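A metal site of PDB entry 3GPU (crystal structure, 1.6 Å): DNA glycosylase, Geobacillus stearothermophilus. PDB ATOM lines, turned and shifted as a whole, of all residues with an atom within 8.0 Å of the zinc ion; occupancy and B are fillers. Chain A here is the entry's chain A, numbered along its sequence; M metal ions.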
ATOM      1  N   PHE A 181      11.886 -18.414  15.677  1.00  0.00           N
ATOM      2  CA  PHE A 181      12.122 -17.523  16.825  1.00  0.00           C
ATOM      3  C   PHE A 181      13.300 -16.586  16.570  1.00  0.00           C
ATOM      4  O   PHE A 181      13.194 -15.363  16.764  1.00  0.00           O
ATOM      5  CB  PHE A 181      12.382 -18.314  18.119  1.00  0.00           C
ATOM      6  CG  PHE A 181      12.849 -17.436  19.244  1.00  0.00           C
ATOM      7  CD1 PHE A 181      11.916 -16.706  19.977  1.00  0.00           C
ATOM      8  CD2 PHE A 181      14.208 -17.256  19.504  1.00  0.00           C
ATOM      9  CE1 PHE A 181      12.322 -15.830  20.993  1.00  0.00           C
ATOM     10  CE2 PHE A 181      14.637 -16.377  20.527  1.00  0.00           C
ATOM     11  CZ  PHE A 181      13.686 -15.672  21.283  1.00  0.00           C
ATOM     12  N   TYR A 222      15.797 -21.770  22.612  1.00  0.00           N
ATOM     13  CA  TYR A 222      15.056 -20.559  22.961  1.00  0.00           C
ATOM     14  C   TYR A 222      13.576 -20.826  23.218  1.00  0.00           C
ATOM     15  O   TYR A 222      12.983 -20.198  24.079  1.00  0.00           O
ATOM     16  CB  TYR A 222      15.165 -19.537  21.836  1.00  0.00           C
ATOM     17  CG  TYR A 222      16.512 -18.916  21.711  1.00  0.00           C
ATOM     18  CD1 TYR A 222      17.367 -19.243  20.648  1.00  0.00           C
ATOM     19  CD2 TYR A 222      16.958 -17.983  22.654  1.00  0.00           C
ATOM     20  CE1 TYR A 222      18.613 -18.648  20.519  1.00  0.00           C
ATOM     21  CE2 TYR A 222      18.206 -17.398  22.548  1.00  0.00           C
ATOM     22  CZ  TYR A 222      19.028 -17.734  21.484  1.00  0.00           C
ATOM     23  OH  TYR A 222      20.259 -17.133  21.383  1.00  0.00           O
ATOM     24  N   VAL A 223      12.982 -21.739  22.457  1.00  0.00           N
ATOM     25  CA  VAL A 223      11.532 -21.938  22.535  1.00  0.00           C
ATOM     26  C   VAL A 223      11.077 -23.400  22.610  1.00  0.00           C
ATOM     27  O   VAL A 223      10.092 -23.690  23.274  1.00  0.00           O
ATOM     28  CB  VAL A 223      10.747 -21.211  21.383  1.00  0.00           C
ATOM     29  CG1 VAL A 223      10.907 -19.696  21.489  1.00  0.00           C
ATOM     30  CG2 VAL A 223      11.181 -21.711  19.983  1.00  0.00           C
ATOM     31  N   PRO A 230       9.980 -18.321  30.808  1.00  0.00           N
ATOM     32  CA  PRO A 230      10.260 -17.015  30.208  1.00  0.00           C
ATOM     33  C   PRO A 230      11.123 -17.094  28.955  1.00  0.00           C
ATOM     34  O   PRO A 230      12.075 -17.873  28.899  1.00  0.00           O
ATOM     35  CB  PRO A 230      11.060 -16.286  31.278  1.00  0.00           C
ATOM     36  CG  PRO A 230      10.713 -16.988  32.546  1.00  0.00           C
ATOM     37  CD  PRO A 230      10.523 -18.404  32.185  1.00  0.00           C
ATOM     38  N   CYS A 231      10.801 -16.269  27.976  1.00  0.00           N
ATOM     39  CA  CYS A 231      11.674 -16.081  26.831  1.00  0.00           C
ATOM     40  C   CYS A 231      13.048 -15.620  27.318  1.00  0.00           C
ATOM     41  O   CYS A 231      13.156 -14.754  28.192  1.00  0.00           O
ATOM     42  CB  CYS A 231      11.074 -15.042  25.891  1.00  0.00           C
ATOM     43  SG  CYS A 231      12.098 -14.664  24.459  1.00  0.00           S
ATOM     44  N   LYS A 232      14.093 -16.237  26.775  1.00  0.00           N
ATOM     45  CA  LYS A 232      15.482 -15.882  27.126  1.00  0.00           C
ATOM     46  C   LYS A 232      15.908 -14.510  26.636  1.00  0.00           C
ATOM     47  O   LYS A 232      16.931 -13.960  27.094  1.00  0.00           O
ATOM     48  CB  LYS A 232      16.457 -16.963  26.618  1.00  0.00           C
ATOM     49  CG  LYS A 232      16.265 -18.300  27.310  1.00  0.00           C
ATOM     50  CD  LYS A 232      17.171 -19.378  26.728  1.00  0.00           C
ATOM     51  CE  LYS A 232      17.034 -20.667  27.546  1.00  0.00           C
ATOM     52  NZ  LYS A 232      17.979 -21.734  27.107  1.00  0.00           N
ATOM     53  N   ARG A 233      15.125 -13.935  25.718  1.00  0.00           N
ATOM     54  CA  ARG A 233      15.442 -12.631  25.127  1.00  0.00           C
ATOM     55  C   ARG A 233      14.604 -11.493  25.709  1.00  0.00           C
ATOM     56  O   ARG A 233      15.087 -10.389  25.816  1.00  0.00           O
ATOM     57  CB  ARG A 233      15.287 -12.668  23.605  1.00  0.00           C
ATOM     58  CG  ARG A 233      16.338 -13.537  22.919  1.00  0.00           C
ATOM     59  CD  ARG A 233      17.538 -12.710  22.507  1.00  0.00           C
ATOM     60  NE  ARG A 233      18.538 -13.518  21.802  1.00  0.00           N
ATOM     61  CZ  ARG A 233      18.500 -13.847  20.513  1.00  0.00           C
ATOM     62  NH1 ARG A 233      17.486 -13.480  19.731  1.00  0.00           N
ATOM     63  NH2 ARG A 233      19.485 -14.578  20.002  1.00  0.00           N
ATOM     64  N   CYS A 234      13.346 -11.776  26.083  1.00  0.00           N
ATOM     65  CA  CYS A 234      12.443 -10.714  26.539  1.00  0.00           C
ATOM     66  C   CYS A 234      11.659 -11.027  27.801  1.00  0.00           C
ATOM     67  O   CYS A 234      10.992 -10.126  28.347  1.00  0.00           O
ATOM     68  CB  CYS A 234      11.460 -10.284  25.428  1.00  0.00           C
ATOM     69  SG  CYS A 234      10.099 -11.480  25.150  1.00  0.00           S
ATOM     70  N   GLY A 235      11.700 -12.267  28.271  1.00  0.00           N
ATOM     71  CA  GLY A 235      11.009 -12.637  29.520  1.00  0.00           C
ATOM     72  C   GLY A 235       9.538 -13.005  29.420  1.00  0.00           C
ATOM     73  O   GLY A 235       8.938 -13.483  30.402  1.00  0.00           O
ATOM     74  N   THR A 236       8.945 -12.800  28.241  1.00  0.00           N
ATOM     75  CA  THR A 236       7.535 -13.132  27.993  1.00  0.00           C
ATOM     76  C   THR A 236       7.408 -14.655  28.017  1.00  0.00           C
ATOM     77  O   THR A 236       8.243 -15.353  27.454  1.00  0.00           O
ATOM     78  CB  THR A 236       7.107 -12.601  26.606  1.00  0.00           C
ATOM     79  OG1 THR A 236       7.239 -11.165  26.580  1.00  0.00           O
ATOM     80  CG2 THR A 236       5.654 -12.983  26.274  1.00  0.00           C
ATOM     81  N   PRO A 237       6.361 -15.189  28.690  1.00  0.00           N
ATOM     82  CA  PRO A 237       6.183 -16.642  28.644  1.00  0.00           C
ATOM     83  C   PRO A 237       6.079 -17.228  27.230  1.00  0.00           C
ATOM     84  O   PRO A 237       5.329 -16.739  26.369  1.00  0.00           O
ATOM     85  CB  PRO A 237       4.861 -16.844  29.400  1.00  0.00           C
ATOM     86  CG  PRO A 237       4.843 -15.714  30.362  1.00  0.00           C
ATOM     87  CD  PRO A 237       5.364 -14.548  29.560  1.00  0.00           C
ATOM     88  N   ILE A 238       6.859 -18.279  26.988  1.00  0.00           N
ATOM     89  CA  ILE A 238       6.792 -19.004  25.719  1.00  0.00           C
ATOM     90  C   ILE A 238       5.435 -19.713  25.628  1.00  0.00           C
ATOM     91  O   ILE A 238       4.930 -20.215  26.644  1.00  0.00           O
ATOM     92  CB  ILE A 238       7.974 -19.988  25.598  1.00  0.00           C
ATOM     93  CG1 ILE A 238       9.298 -19.205  25.591  1.00  0.00           C
ATOM     94  CG2 ILE A 238       7.840 -20.889  24.363  1.00  0.00           C
ATOM     95  CD1 ILE A 238       9.338 -18.003  24.588  1.00  0.00           C
ATOM     96  N   TYR A 250       6.613 -20.708  20.489  1.00  0.00           N
ATOM     97  CA  TYR A 250       6.984 -19.378  20.020  1.00  0.00           C
ATOM     98  C   TYR A 250       6.904 -18.347  21.139  1.00  0.00           C
ATOM     99  O   TYR A 250       6.214 -18.554  22.152  1.00  0.00           O
ATOM    100  CB  TYR A 250       6.067 -18.965  18.849  1.00  0.00           C
ATOM    101  CG  TYR A 250       4.627 -18.877  19.266  1.00  0.00           C
ATOM    102  CD1 TYR A 250       4.077 -17.651  19.659  1.00  0.00           C
ATOM    103  CD2 TYR A 250       3.812 -20.012  19.308  1.00  0.00           C
ATOM    104  CE1 TYR A 250       2.760 -17.557  20.082  1.00  0.00           C
ATOM    105  CE2 TYR A 250       2.488 -19.914  19.752  1.00  0.00           C
ATOM    106  CZ  TYR A 250       1.962 -18.687  20.124  1.00  0.00           C
ATOM    107  OH  TYR A 250       0.663 -18.567  20.553  1.00  0.00           O
ATOM    108  N   CYS A 251       7.630 -17.247  20.960  1.00  0.00           N
ATOM    109  CA  CYS A 251       7.466 -16.096  21.850  1.00  0.00           C
ATOM    110  C   CYS A 251       6.553 -15.102  21.160  1.00  0.00           C
ATOM    111  O   CYS A 251       6.871 -14.628  20.066  1.00  0.00           O
ATOM    112  CB  CYS A 251       8.814 -15.419  22.126  1.00  0.00           C
ATOM    113  SG  CYS A 251       8.578 -13.917  23.107  1.00  0.00           S
ATOM    114  N   PRO A 252       5.408 -14.755  21.790  1.00  0.00           N
ATOM    115  CA  PRO A 252       4.486 -13.864  21.105  1.00  0.00           C
ATOM    116  C   PRO A 252       4.933 -12.398  21.064  1.00  0.00           C
ATOM    117  O   PRO A 252       4.258 -11.588  20.416  1.00  0.00           O
ATOM    118  CB  PRO A 252       3.189 -14.009  21.924  1.00  0.00           C
ATOM    119  CG  PRO A 252       3.691 -14.322  23.310  1.00  0.00           C
ATOM    120  CD  PRO A 252       4.841 -15.257  23.058  1.00  0.00           C
ATOM    121  N   ARG A 253       6.007 -12.052  21.770  1.00  0.00           N
ATOM    122  CA  ARG A 253       6.581 -10.700  21.670  1.00  0.00           C
ATOM    123  C   ARG A 253       7.708 -10.604  20.633  1.00  0.00           C
ATOM    124  O   ARG A 253       7.724  -9.676  19.813  1.00  0.00           O
ATOM    125  CB  ARG A 253       7.077 -10.210  23.022  1.00  0.00           C
ATOM    126  CG  ARG A 253       7.742  -8.848  22.968  1.00  0.00           C
ATOM    127  CD  ARG A 253       8.090  -8.322  24.360  1.00  0.00           C
ATOM    128  NE  ARG A 253       8.658  -6.990  24.233  1.00  0.00           N
ATOM    129  CZ  ARG A 253       9.038  -6.221  25.253  1.00  0.00           C
ATOM    130  NH1 ARG A 253       9.486  -4.987  25.026  1.00  0.00           N
ATOM    131  NH2 ARG A 253       8.972  -6.678  26.514  1.00  0.00           N
ATOM    132  N   CYS A 254       8.652 -11.547  20.684  1.00  0.00           N
ATOM    133  CA  CYS A 254       9.821 -11.516  19.780  1.00  0.00           C
ATOM    134  C   CYS A 254       9.433 -11.836  18.347  1.00  0.00           C
ATOM    135  O   CYS A 254      10.081 -11.365  17.389  1.00  0.00           O
ATOM    136  CB  CYS A 254      10.860 -12.555  20.258  1.00  0.00           C
ATOM    137  SG  CYS A 254      11.784 -12.030  21.728  1.00  0.00           S
ATOM    138  N   GLN A 255       8.367 -12.626  18.189  1.00  0.00           N
ATOM    139  CA  GLN A 255       7.951 -13.102  16.869  1.00  0.00           C
ATOM    140  C   GLN A 255       6.698 -12.388  16.411  1.00  0.00           C
ATOM    141  O   GLN A 255       5.742 -12.215  17.194  1.00  0.00           O
ATOM    142  CB  GLN A 255       7.734 -14.624  16.888  1.00  0.00           C
ATOM    143  CG  GLN A 255       9.033 -15.385  17.080  1.00  0.00           C
ATOM    144  CD  GLN A 255       8.825 -16.859  17.360  1.00  0.00           C
ATOM    145  OE1 GLN A 255       8.956 -17.298  18.487  1.00  0.00           O
ATOM    146  NE2 GLN A 255       8.563 -17.641  16.303  1.00  0.00           N
HETATM  147 ZN    ZN M   1      10.698 -13.034  23.529  1.00  0.00          ZN
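The side-chain sulfur (SG) of Cys 234 lies close to the side-chain hydroxyl (OG1) of Thr 236 (3.2 Å).
SG of Cys 251 sits close to N of Arg 253, 3.4 Å away.
N of Cys 251 is in hydrogen-bond range of OE1 of Gln 255 (2.8 Å).
The side-chain sulfur of Cys 231 sits close to the backbone NH of Arg 233 (3.4 Å).
O of Thr 236 sits at hydrogen-bond distance from N of Cys 231.
Four residues have an atom within 4 Å of the zinc ion: Cys 231, Cys 234, Cys 251 and Cys 254.
SG of Cys 234 binds the zinc ion.
SG of Cys 254 binds the zinc ion, 2.3 Å away.
SG of Cys 251 binds the zinc ion, 2.3 Å away.
The zinc ion is bound by SG of Cys 231.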
